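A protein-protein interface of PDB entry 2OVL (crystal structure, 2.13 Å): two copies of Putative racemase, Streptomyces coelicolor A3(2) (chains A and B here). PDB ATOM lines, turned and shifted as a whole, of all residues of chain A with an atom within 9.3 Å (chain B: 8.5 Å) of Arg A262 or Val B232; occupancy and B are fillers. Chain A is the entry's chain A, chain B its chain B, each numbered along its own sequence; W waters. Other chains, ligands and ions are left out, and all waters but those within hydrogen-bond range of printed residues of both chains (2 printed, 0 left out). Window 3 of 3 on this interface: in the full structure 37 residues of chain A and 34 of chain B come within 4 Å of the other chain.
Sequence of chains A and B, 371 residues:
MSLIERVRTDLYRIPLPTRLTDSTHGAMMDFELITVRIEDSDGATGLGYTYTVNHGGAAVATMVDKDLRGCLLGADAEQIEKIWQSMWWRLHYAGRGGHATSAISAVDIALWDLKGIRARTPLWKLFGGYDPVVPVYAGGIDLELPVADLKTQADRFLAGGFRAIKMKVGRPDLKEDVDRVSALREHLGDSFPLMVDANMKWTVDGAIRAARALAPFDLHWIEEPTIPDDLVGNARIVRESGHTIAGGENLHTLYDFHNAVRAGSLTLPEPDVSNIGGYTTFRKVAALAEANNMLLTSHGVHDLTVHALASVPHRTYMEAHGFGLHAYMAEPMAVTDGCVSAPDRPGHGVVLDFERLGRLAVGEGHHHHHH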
ATOM      1  N   LEU A 231     -37.270   8.069   8.362  1.00  0.00           N
ATOM      2  CA  LEU A 231     -37.365   9.488   8.044  1.00  0.00           C
ATOM      3  C   LEU A 231     -38.163   9.746   6.762  1.00  0.00           C
ATOM      4  O   LEU A 231     -39.034  10.620   6.732  1.00  0.00           O
ATOM      5  CB  LEU A 231     -35.962  10.093   7.912  1.00  0.00           C
ATOM      6  CG  LEU A 231     -35.076  10.036   9.160  1.00  0.00           C
ATOM      7  CD1 LEU A 231     -33.672  10.551   8.834  1.00  0.00           C
ATOM      8  CD2 LEU A 231     -35.711  10.871  10.272  1.00  0.00           C
ATOM      9  N   ALA A 235     -41.869  11.594   6.585  1.00  0.00           N
ATOM     10  CA  ALA A 235     -41.933  12.839   5.820  1.00  0.00           C
ATOM     11  C   ALA A 235     -43.120  12.730   4.870  1.00  0.00           C
ATOM     12  O   ALA A 235     -43.811  13.707   4.600  1.00  0.00           O
ATOM     13  CB  ALA A 235     -40.634  13.041   5.013  1.00  0.00           C
ATOM     14  N   LEU A 254     -29.718  14.232  20.236  1.00  0.00           N
ATOM     15  CA  LEU A 254     -29.954  15.510  19.601  1.00  0.00           C
ATOM     16  C   LEU A 254     -29.940  15.274  18.085  1.00  0.00           C
ATOM     17  O   LEU A 254     -30.715  15.872  17.352  1.00  0.00           O
ATOM     18  CB  LEU A 254     -28.840  16.483  20.003  1.00  0.00           C
ATOM     19  CG  LEU A 254     -28.794  17.875  19.379  1.00  0.00           C
ATOM     20  CD1 LEU A 254     -30.081  18.636  19.686  1.00  0.00           C
ATOM     21  CD2 LEU A 254     -27.578  18.610  19.921  1.00  0.00           C
ATOM     22  N   TYR A 255     -29.068  14.382  17.623  1.00  0.00           N
ATOM     23  CA  TYR A 255     -28.971  14.096  16.188  1.00  0.00           C
ATOM     24  C   TYR A 255     -30.255  13.499  15.608  1.00  0.00           C
ATOM     25  O   TYR A 255     -30.610  13.802  14.465  1.00  0.00           O
ATOM     26  CB  TYR A 255     -27.781  13.174  15.921  1.00  0.00           C
ATOM     27  CG  TYR A 255     -26.509  13.643  16.596  1.00  0.00           C
ATOM     28  CD1 TYR A 255     -25.928  14.874  16.274  1.00  0.00           C
ATOM     29  CD2 TYR A 255     -25.908  12.873  17.595  1.00  0.00           C
ATOM     30  CE1 TYR A 255     -24.772  15.325  16.939  1.00  0.00           C
ATOM     31  CE2 TYR A 255     -24.768  13.313  18.263  1.00  0.00           C
ATOM     32  CZ  TYR A 255     -24.201  14.535  17.937  1.00  0.00           C
ATOM     33  OH  TYR A 255     -23.075  14.954  18.622  1.00  0.00           O
ATOM     34  N   ASP A 256     -30.949  12.658  16.385  1.00  0.00           N
ATOM     35  CA  ASP A 256     -32.212  12.063  15.928  1.00  0.00           C
ATOM     36  C   ASP A 256     -33.207  13.175  15.609  1.00  0.00           C
ATOM     37  O   ASP A 256     -33.895  13.133  14.593  1.00  0.00           O
ATOM     38  CB  ASP A 256     -32.858  11.172  17.006  1.00  0.00           C
ATOM     39  CG  ASP A 256     -32.277   9.767  17.057  1.00  0.00           C
ATOM     40  OD1 ASP A 256     -31.660   9.318  16.064  1.00  0.00           O
ATOM     41  OD2 ASP A 256     -32.468   9.098  18.100  1.00  0.00           O
ATOM     42  N   PHE A 257     -33.295  14.156  16.505  1.00  0.00           N
ATOM     43  CA  PHE A 257     -34.213  15.280  16.326  1.00  0.00           C
ATOM     44  C   PHE A 257     -33.781  16.159  15.163  1.00  0.00           C
ATOM     45  O   PHE A 257     -34.611  16.676  14.422  1.00  0.00           O
ATOM     46  CB  PHE A 257     -34.301  16.100  17.620  1.00  0.00           C
ATOM     47  CG  PHE A 257     -35.367  15.616  18.569  1.00  0.00           C
ATOM     48  CD1 PHE A 257     -36.701  15.944  18.358  1.00  0.00           C
ATOM     49  CD2 PHE A 257     -35.041  14.803  19.649  1.00  0.00           C
ATOM     50  CE1 PHE A 257     -37.703  15.468  19.212  1.00  0.00           C
ATOM     51  CE2 PHE A 257     -36.029  14.319  20.508  1.00  0.00           C
ATOM     52  CZ  PHE A 257     -37.369  14.653  20.290  1.00  0.00           C
ATOM     53  N   HIS A 258     -32.474  16.318  15.011  1.00  0.00           N
ATOM     54  CA  HIS A 258     -31.910  17.103  13.924  1.00  0.00           C
ATOM     55  C   HIS A 258     -32.328  16.453  12.598  1.00  0.00           C
ATOM     56  O   HIS A 258     -32.825  17.134  11.695  1.00  0.00           O
ATOM     57  CB  HIS A 258     -30.383  17.130  14.051  1.00  0.00           C
ATOM     58  CG  HIS A 258     -29.689  17.759  12.885  1.00  0.00           C
ATOM     59  ND1 HIS A 258     -29.862  19.082  12.541  1.00  0.00           N
ATOM     60  CD2 HIS A 258     -28.831  17.242  11.973  1.00  0.00           C
ATOM     61  CE1 HIS A 258     -29.142  19.353  11.468  1.00  0.00           C
ATOM     62  NE2 HIS A 258     -28.507  18.255  11.103  1.00  0.00           N
ATOM     63  N   ASN A 259     -32.134  15.139  12.494  1.00  0.00           N
ATOM     64  CA  ASN A 259     -32.510  14.392  11.289  1.00  0.00           C
ATOM     65  C   ASN A 259     -33.985  14.561  10.979  1.00  0.00           C
ATOM     66  O   ASN A 259     -34.356  14.882   9.854  1.00  0.00           O
ATOM     67  CB  ASN A 259     -32.273  12.880  11.448  1.00  0.00           C
ATOM     68  CG  ASN A 259     -30.813  12.508  11.482  1.00  0.00           C
ATOM     69  OD1 ASN A 259     -29.944  13.282  11.080  1.00  0.00           O
ATOM     70  ND2 ASN A 259     -30.535  11.297  11.952  1.00  0.00           N
ATOM     71  N   ALA A 260     -34.828  14.312  11.979  1.00  0.00           N
ATOM     72  CA  ALA A 260     -36.272  14.411  11.783  1.00  0.00           C
ATOM     73  C   ALA A 260     -36.697  15.801  11.337  1.00  0.00           C
ATOM     74  O   ALA A 260     -37.491  15.948  10.408  1.00  0.00           O
ATOM     75  CB  ALA A 260     -37.022  14.014  13.071  1.00  0.00           C
ATOM     76  N   VAL A 261     -36.176  16.823  12.010  1.00  0.00           N
ATOM     77  CA  VAL A 261     -36.516  18.202  11.671  1.00  0.00           C
ATOM     78  C   VAL A 261     -36.037  18.545  10.262  1.00  0.00           C
ATOM     79  O   VAL A 261     -36.792  19.083   9.449  1.00  0.00           O
ATOM     80  CB  VAL A 261     -35.890  19.180  12.694  1.00  0.00           C
ATOM     81  CG1 VAL A 261     -36.113  20.622  12.259  1.00  0.00           C
ATOM     82  CG2 VAL A 261     -36.518  18.947  14.062  1.00  0.00           C
ATOM     83  N   ARG A 262     -34.786  18.205   9.969  1.00  0.00           N
ATOM     84  CA  ARG A 262     -34.213  18.484   8.665  1.00  0.00           C
ATOM     85  C   ARG A 262     -34.963  17.748   7.555  1.00  0.00           C
ATOM     86  O   ARG A 262     -35.139  18.288   6.462  1.00  0.00           O
ATOM     87  CB  ARG A 262     -32.731  18.100   8.658  1.00  0.00           C
ATOM     88  CG  ARG A 262     -31.994  18.506   7.402  1.00  0.00           C
ATOM     89  CD  ARG A 262     -30.517  18.133   7.471  1.00  0.00           C
ATOM     90  NE  ARG A 262     -29.901  18.204   6.148  1.00  0.00           N
ATOM     91  CZ  ARG A 262     -29.435  19.312   5.582  1.00  0.00           C
ATOM     92  NH1 ARG A 262     -29.499  20.477   6.218  1.00  0.00           N
ATOM     93  NH2 ARG A 262     -28.900  19.250   4.367  1.00  0.00           N
ATOM     94  N   ALA A 263     -35.417  16.528   7.833  1.00  0.00           N
ATOM     95  CA  ALA A 263     -36.158  15.755   6.841  1.00  0.00           C
ATOM     96  C   ALA A 263     -37.648  16.120   6.794  1.00  0.00           C
ATOM     97  O   ALA A 263     -38.375  15.666   5.910  1.00  0.00           O
ATOM     98  CB  ALA A 263     -36.007  14.269   7.127  1.00  0.00           C
ATOM     99  N   GLY A 264     -38.104  16.943   7.735  1.00  0.00           N
ATOM    100  CA  GLY A 264     -39.510  17.308   7.769  1.00  0.00           C
ATOM    101  C   GLY A 264     -40.359  16.070   8.033  1.00  0.00           C
ATOM    102  O   GLY A 264     -41.462  15.915   7.497  1.00  0.00           O
ATOM    103  N   SER A 265     -39.841  15.180   8.872  1.00  0.00           N
ATOM    104  CA  SER A 265     -40.545  13.955   9.184  1.00  0.00           C
ATOM    105  C   SER A 265     -41.482  14.087  10.390  1.00  0.00           C
ATOM    106  O   SER A 265     -42.076  13.114  10.838  1.00  0.00           O
ATOM    107  CB  SER A 265     -39.540  12.809   9.359  1.00  0.00           C
ATOM    108  OG  SER A 265     -38.580  13.104  10.350  1.00  0.00           O
ATOM    109  N   LEU A 266     -41.611  15.305  10.905  1.00  0.00           N
ATOM    110  CA  LEU A 266     -42.528  15.598  12.010  1.00  0.00           C
ATOM    111  C   LEU A 266     -42.759  17.107  12.031  1.00  0.00           C
ATOM    112  O   LEU A 266     -41.905  17.872  11.577  1.00  0.00           O
ATOM    113  CB  LEU A 266     -41.962  15.109  13.352  1.00  0.00           C
ATOM    114  CG  LEU A 266     -40.627  15.625  13.905  1.00  0.00           C
ATOM    115  CD1 LEU A 266     -40.738  17.089  14.305  1.00  0.00           C
ATOM    116  CD2 LEU A 266     -40.254  14.780  15.121  1.00  0.00           C
ATOM    117  N   LEU A 288     -33.568  23.905  18.647  1.00  0.00           N
ATOM    118  CA  LEU A 288     -33.740  23.477  17.256  1.00  0.00           C
ATOM    119  C   LEU A 288     -35.160  23.768  16.802  1.00  0.00           C
ATOM    120  O   LEU A 288     -35.383  24.273  15.702  1.00  0.00           O
ATOM    121  CB  LEU A 288     -33.487  21.979  17.101  1.00  0.00           C
ATOM    122  CG  LEU A 288     -32.079  21.443  17.343  1.00  0.00           C
ATOM    123  CD1 LEU A 288     -32.028  19.954  16.948  1.00  0.00           C
ATOM    124  CD2 LEU A 288     -31.082  22.240  16.510  1.00  0.00           C
ATOM    125  N   ASN A 292     -36.590  26.464  13.912  1.00  0.00           N
ATOM    126  CA  ASN A 292     -37.408  25.999  12.794  1.00  0.00           C
ATOM    127  C   ASN A 292     -38.860  26.450  12.855  1.00  0.00           C
ATOM    128  O   ASN A 292     -39.705  25.909  12.148  1.00  0.00           O
ATOM    129  CB  ASN A 292     -37.352  24.475  12.735  1.00  0.00           C
ATOM    130  CG  ASN A 292     -36.049  23.963  12.165  1.00  0.00           C
ATOM    131  OD1 ASN A 292     -35.934  23.758  10.955  1.00  0.00           O
ATOM    132  ND2 ASN A 292     -35.051  23.766  13.027  1.00  0.00           N
ATOM    133  N   MET A 294     -41.148  26.038  15.178  1.00  0.00           N
ATOM    134  CA  MET A 294     -42.010  24.948  15.610  1.00  0.00           C
ATOM    135  C   MET A 294     -42.368  25.144  17.079  1.00  0.00           C
ATOM    136  O   MET A 294     -41.634  25.797  17.817  1.00  0.00           O
ATOM    137  CB  MET A 294     -41.292  23.599  15.493  1.00  0.00           C
ATOM    138  CG  MET A 294     -40.895  23.179  14.081  1.00  0.00           C
ATOM    139  SD  MET A 294     -39.920  21.499  14.135  1.00  0.00           S
ATOM    140  CE  MET A 294     -38.155  22.113  14.533  1.00  0.00           C
ATOM    141  N   VAL B 204     -15.614  17.740  10.457  1.00  0.00           N
ATOM    142  CA  VAL B 204     -15.830  17.592   9.026  1.00  0.00           C
ATOM    143  C   VAL B 204     -14.712  18.302   8.259  1.00  0.00           C
ATOM    144  O   VAL B 204     -14.059  17.687   7.406  1.00  0.00           O
ATOM    145  CB  VAL B 204     -17.201  18.166   8.610  1.00  0.00           C
ATOM    146  CG1 VAL B 204     -17.336  18.153   7.093  1.00  0.00           C
ATOM    147  CG2 VAL B 204     -18.315  17.339   9.246  1.00  0.00           C
ATOM    148  N   ILE B 208     -11.510  16.589   5.943  1.00  0.00           N
ATOM    149  CA  ILE B 208     -11.230  16.889   4.545  1.00  0.00           C
ATOM    150  C   ILE B 208      -9.783  17.360   4.445  1.00  0.00           C
ATOM    151  O   ILE B 208      -9.056  16.971   3.539  1.00  0.00           O
ATOM    152  CB  ILE B 208     -12.215  17.963   4.014  1.00  0.00           C
ATOM    153  CG1 ILE B 208     -13.631  17.367   3.976  1.00  0.00           C
ATOM    154  CG2 ILE B 208     -11.785  18.460   2.624  1.00  0.00           C
ATOM    155  CD1 ILE B 208     -14.713  18.369   3.638  1.00  0.00           C
ATOM    156  N   THR B 226     -15.280  11.274  11.123  1.00  0.00           N
ATOM    157  CA  THR B 226     -15.920  12.064  12.174  1.00  0.00           C
ATOM    158  C   THR B 226     -17.051  11.233  12.807  1.00  0.00           C
ATOM    159  O   THR B 226     -17.144  10.027  12.554  1.00  0.00           O
ATOM    160  CB  THR B 226     -16.479  13.405  11.611  1.00  0.00           C
ATOM    161  OG1 THR B 226     -16.943  14.225  12.694  1.00  0.00           O
ATOM    162  CG2 THR B 226     -17.630  13.152  10.637  1.00  0.00           C
ATOM    163  N   ILE B 227     -17.899  11.840  13.631  1.00  0.00           N
ATOM    164  CA  ILE B 227     -18.969  11.053  14.247  1.00  0.00           C
ATOM    165  C   ILE B 227     -19.961  10.540  13.209  1.00  0.00           C
ATOM    166  O   ILE B 227     -20.267  11.221  12.232  1.00  0.00           O
ATOM    167  CB  ILE B 227     -19.726  11.833  15.348  1.00  0.00           C
ATOM    168  CG1 ILE B 227     -20.341  13.109  14.776  1.00  0.00           C
ATOM    169  CG2 ILE B 227     -18.765  12.138  16.510  1.00  0.00           C
ATOM    170  CD1 ILE B 227     -21.141  13.901  15.799  1.00  0.00           C
ATOM    171  N   PRO B 228     -20.471   9.315  13.413  1.00  0.00           N
ATOM    172  CA  PRO B 228     -21.423   8.686  12.498  1.00  0.00           C
ATOM    173  C   PRO B 228     -22.808   9.312  12.430  1.00  0.00           C
ATOM    174  O   PRO B 228     -23.496   9.182  11.428  1.00  0.00           O
ATOM    175  CB  PRO B 228     -21.457   7.239  12.988  1.00  0.00           C
ATOM    176  CG  PRO B 228     -21.238   7.377  14.453  1.00  0.00           C
ATOM    177  CD  PRO B 228     -20.113   8.397  14.510  1.00  0.00           C
ATOM    178  N   ASP B 229     -23.202  10.004  13.490  1.00  0.00           N
ATOM    179  CA  ASP B 229     -24.524  10.620  13.564  1.00  0.00           C
ATOM    180  C   ASP B 229     -24.756  11.720  12.536  1.00  0.00           C
ATOM    181  O   ASP B 229     -25.900  12.025  12.191  1.00  0.00           O
ATOM    182  CB  ASP B 229     -24.731  11.219  14.956  1.00  0.00           C
ATOM    183  CG  ASP B 229     -24.273  10.299  16.059  1.00  0.00           C
ATOM    184  OD1 ASP B 229     -25.133   9.691  16.733  1.00  0.00           O
ATOM    185  OD2 ASP B 229     -23.047  10.184  16.243  1.00  0.00           O
ATOM    186  N   ASP B 230     -23.670  12.317  12.055  1.00  0.00           N
ATOM    187  CA  ASP B 230     -23.758  13.424  11.109  1.00  0.00           C
ATOM    188  C   ASP B 230     -23.795  12.981   9.640  1.00  0.00           C
ATOM    189  O   ASP B 230     -22.763  12.874   8.983  1.00  0.00           O
ATOM    190  CB  ASP B 230     -22.582  14.369  11.383  1.00  0.00           C
ATOM    191  CG  ASP B 230     -22.519  15.535  10.424  1.00  0.00           C
ATOM    192  OD1 ASP B 230     -23.568  15.916   9.860  1.00  0.00           O
ATOM    193  OD2 ASP B 230     -21.404  16.082  10.255  1.00  0.00           O
ATOM    194  N   LEU B 231     -24.996  12.730   9.131  1.00  0.00           N
ATOM    195  CA  LEU B 231     -25.171  12.287   7.748  1.00  0.00           C
ATOM    196  C   LEU B 231     -24.710  13.345   6.739  1.00  0.00           C
ATOM    197  O   LEU B 231     -24.001  13.038   5.782  1.00  0.00           O
ATOM    198  CB  LEU B 231     -26.646  11.934   7.500  1.00  0.00           C
ATOM    199  CG  LEU B 231     -27.242  10.798   8.350  1.00  0.00           C
ATOM    200  CD1 LEU B 231     -28.767  10.793   8.258  1.00  0.00           C
ATOM    201  CD2 LEU B 231     -26.671   9.473   7.890  1.00  0.00           C
ATOM    202  N   VAL B 232     -25.112  14.590   6.965  1.00  0.00           N
ATOM    203  CA  VAL B 232     -24.754  15.699   6.083  1.00  0.00           C
ATOM    204  C   VAL B 232     -23.242  15.922   6.016  1.00  0.00           C
ATOM    205  O   VAL B 232     -22.663  15.991   4.932  1.00  0.00           O
ATOM    206  CB  VAL B 232     -25.444  17.010   6.554  1.00  0.00           C
ATOM    207  CG1 VAL B 232     -24.963  18.204   5.716  1.00  0.00           C
ATOM    208  CG2 VAL B 232     -26.954  16.861   6.434  1.00  0.00           C
ATOM    209  N   GLY B 233     -22.616  16.044   7.183  1.00  0.00           N
ATOM    210  CA  GLY B 233     -21.183  16.252   7.243  1.00  0.00           C
ATOM    211  C   GLY B 233     -20.406  15.102   6.634  1.00  0.00           C
ATOM    212  O   GLY B 233     -19.427  15.316   5.922  1.00  0.00           O
ATOM    213  N   ASN B 234     -20.831  13.875   6.913  1.00  0.00           N
ATOM    214  CA  ASN B 234     -20.145  12.710   6.360  1.00  0.00           C
ATOM    215  C   ASN B 234     -20.274  12.645   4.841  1.00  0.00           C
ATOM    216  O   ASN B 234     -19.336  12.245   4.147  1.00  0.00           O
ATOM    217  CB  ASN B 234     -20.680  11.427   7.007  1.00  0.00           C
ATOM    218  CG  ASN B 234     -19.998  11.126   8.323  1.00  0.00           C
ATOM    219  OD1 ASN B 234     -18.825  10.761   8.345  1.00  0.00           O
ATOM    220  ND2 ASN B 234     -20.720  11.301   9.430  1.00  0.00           N
ATOM    221  N   ALA B 235     -21.430  13.043   4.324  1.00  0.00           N
ATOM    222  CA  ALA B 235     -21.646  13.046   2.878  1.00  0.00           C
ATOM    223  C   ALA B 235     -20.721  14.083   2.246  1.00  0.00           C
ATOM    224  O   ALA B 235     -20.264  13.918   1.120  1.00  0.00           O
ATOM    225  CB  ALA B 235     -23.107  13.378   2.556  1.00  0.00           C
ATOM    226  N   ARG B 236     -20.443  15.154   2.981  1.00  0.00           N
ATOM    227  CA  ARG B 236     -19.557  16.193   2.474  1.00  0.00           C
ATOM    228  C   ARG B 236     -18.121  15.655   2.428  1.00  0.00           C
ATOM    229  O   ARG B 236     -17.373  15.929   1.493  1.00  0.00           O
ATOM    230  CB  ARG B 236     -19.649  17.439   3.357  1.00  0.00           C
ATOM    231  CG  ARG B 236     -18.800  18.595   2.867  1.00  0.00           C
ATOM    232  CD  ARG B 236     -18.984  19.825   3.739  1.00  0.00           C
ATOM    233  NE  ARG B 236     -17.756  20.606   3.741  1.00  0.00           N
ATOM    234  CZ  ARG B 236     -17.276  21.233   4.805  1.00  0.00           C
ATOM    235  NH1 ARG B 236     -17.925  21.182   5.963  1.00  0.00           N
ATOM    236  NH2 ARG B 236     -16.124  21.882   4.712  1.00  0.00           N
ATOM    237  N   ILE B 237     -17.738  14.880   3.434  1.00  0.00           N
ATOM    238  CA  ILE B 237     -16.397  14.294   3.454  1.00  0.00           C
ATOM    239  C   ILE B 237     -16.270  13.344   2.254  1.00  0.00           C
ATOM    240  O   ILE B 237     -15.248  13.323   1.559  1.00  0.00           O
ATOM    241  CB  ILE B 237     -16.157  13.518   4.774  1.00  0.00           C
ATOM    242  CG1 ILE B 237     -16.215  14.492   5.957  1.00  0.00           C
ATOM    243  CG2 ILE B 237     -14.809  12.788   4.726  1.00  0.00           C
ATOM    244  CD1 ILE B 237     -16.073  13.825   7.332  1.00  0.00           C
ATOM    245  N   VAL B 238     -17.316  12.565   2.002  1.00  0.00           N
ATOM    246  CA  VAL B 238     -17.305  11.646   0.868  1.00  0.00           C
ATOM    247  C   VAL B 238     -17.067  12.420  -0.437  1.00  0.00           C
ATOM    248  O   VAL B 238     -16.211  12.068  -1.243  1.00  0.00           O
ATOM    249  CB  VAL B 238     -18.646  10.872   0.772  1.00  0.00           C
ATOM    250  CG1 VAL B 238     -18.713  10.081  -0.533  1.00  0.00           C
ATOM    251  CG2 VAL B 238     -18.775   9.923   1.954  1.00  0.00           C
ATOM    252  N   ARG B 239     -17.817  13.494  -0.624  1.00  0.00           N
ATOM    253  CA  ARG B 239     -17.706  14.317  -1.818  1.00  0.00           C
ATOM    254  C   ARG B 239     -16.365  15.027  -1.999  1.00  0.00           C
ATOM    255  O   ARG B 239     -15.904  15.203  -3.128  1.00  0.00           O
ATOM    256  CB  ARG B 239     -18.816  15.372  -1.816  1.00  0.00           C
ATOM    257  CG  ARG B 239     -20.221  14.821  -1.995  1.00  0.00           C
ATOM    258  CD  ARG B 239     -21.274  15.922  -1.841  1.00  0.00           C
ATOM    259  NE  ARG B 239     -20.814  17.187  -2.407  1.00  0.00           N
ATOM    260  CZ  ARG B 239     -20.176  18.128  -1.716  1.00  0.00           C
ATOM    261  NH1 ARG B 239     -19.931  17.949  -0.425  1.00  0.00           N
ATOM    262  NH2 ARG B 239     -19.760  19.235  -2.318  1.00  0.00           N
ATOM    263  N   ASN B 259     -29.916   4.887   6.308  1.00  0.00           N
ATOM    264  CA  ASN B 259     -29.718   6.340   6.293  1.00  0.00           C
ATOM    265  C   ASN B 259     -28.394   6.734   5.662  1.00  0.00           C
ATOM    266  O   ASN B 259     -28.346   7.570   4.760  1.00  0.00           O
ATOM    267  CB  ASN B 259     -29.730   6.924   7.715  1.00  0.00           C
ATOM    268  CG  ASN B 259     -31.118   6.980   8.322  1.00  0.00           C
ATOM    269  OD1 ASN B 259     -32.126   6.869   7.623  1.00  0.00           O
ATOM    270  ND2 ASN B 259     -31.173   7.172   9.636  1.00  0.00           N
ATOM    271  N   ALA B 260     -27.315   6.142   6.168  1.00  0.00           N
ATOM    272  CA  ALA B 260     -25.974   6.451   5.688  1.00  0.00           C
ATOM    273  C   ALA B 260     -25.822   6.180   4.198  1.00  0.00           C
ATOM    274  O   ALA B 260     -25.281   7.007   3.455  1.00  0.00           O
ATOM    275  CB  ALA B 260     -24.938   5.653   6.482  1.00  0.00           C
ATOM    276  N   ALA B 263     -27.992   8.706   2.080  1.00  0.00           N
ATOM    277  CA  ALA B 263     -27.423  10.047   2.039  1.00  0.00           C
ATOM    278  C   ALA B 263     -26.022  10.061   1.432  1.00  0.00           C
ATOM    279  O   ALA B 263     -25.453  11.122   1.224  1.00  0.00           O
ATOM    280  CB  ALA B 263     -27.380  10.641   3.444  1.00  0.00           C
ATOM    281  N   GLY B 264     -25.477   8.884   1.136  1.00  0.00           N
ATOM    282  CA  GLY B 264     -24.135   8.806   0.580  1.00  0.00           C
ATOM    283  C   GLY B 264     -23.084   9.285   1.580  1.00  0.00           C
ATOM    284  O   GLY B 264     -22.081   9.894   1.201  1.00  0.00           O
ATOM    285  N   SER B 265     -23.301   9.001   2.863  1.00  0.00           N
ATOM    286  CA  SER B 265     -22.369   9.442   3.892  1.00  0.00           C
ATOM    287  C   SER B 265     -21.173   8.511   4.115  1.00  0.00           C
ATOM    288  O   SER B 265     -20.350   8.738   5.003  1.00  0.00           O
ATOM    289  CB  SER B 265     -23.127   9.679   5.205  1.00  0.00           C
ATOM    290  OG  SER B 265     -23.741   8.492   5.669  1.00  0.00           O
HETATM  291  O   HOH W   1     -28.058  10.043  12.200  1.00  0.00           O
HETATM  292  O   HOH W   2     -27.641  14.329  12.376  1.00  0.00           O
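The backbone carbonyl oxygen of Tyr A255 sits close to the side-chain amide oxygen of Asn A259 (3.5 Å). The backbone carbonyl oxygen of Ile B227 lies within hydrogen-bond range of the side-chain amide nitrogen of Asn B234, at 2.8 Å.
Among the printed residues, merely in contact across the chains: Tyr A255 with Ile B227 (3.6 Å), Tyr A255 with Asp B229 (3.3 Å), Asn A259 with Leu B231 (3.9 Å) and Arg A262 with Val B232 (3.3 Å).
Printed residues of chain B within 4 Å of Tyr A255: Ile B227 (3.6 Å) and Asp B229 (3.3 Å). Of the printed residues of chain B, Asn A259 touches Leu B231. Arg A262 touches just one residue of chain B: Val B232 (3.3 Å). No residue of chain B comes within 4 Å of Ala A263. Ile B208 touches none of the printed residues of chain A. Printed residues of chain A within 4 Å of Ile B227: Tyr A255 (3.6 Å). Printed residues of chain A within 4 Å of Asp B229: Tyr A255. Of the printed residues of chain A, Leu B231 touches Asn A259. Of chain A, only Arg A262 (3.3 Å) comes within 4 Å of Val B232. No residue of chain A comes within 4 Å of Gly B233. No residue of chain A comes within 4 Å of Ala B235. The nearest residue of chain B that does not touch Arg A262 is Leu B231 (7.1 Å). The nearest residue of chain A that does not touch Val B232 is His A258 (5.1 Å).
Of the 21 printed residues of chain B, 4 touch a printed residue of chain A. Hydrophobic or aromatic side chains of chain A within 4 Å of the printed part of chain B: Tyr A255.
Asn A259 touches Leu B231, but with the chains exchanged Leu A231 does not touch Asn B259 (4.2 Å).
Water W1 lies within hydrogen-bond range of the side-chain amide nitrogen (ND2) of Asn A259 and the backbone carbonyl oxygen (O) of Asp B229. Water W2 lies within hydrogen-bond range of OD1 of Asn A259 (2.8 Å) and O of Asp B229 (2.9 Å).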
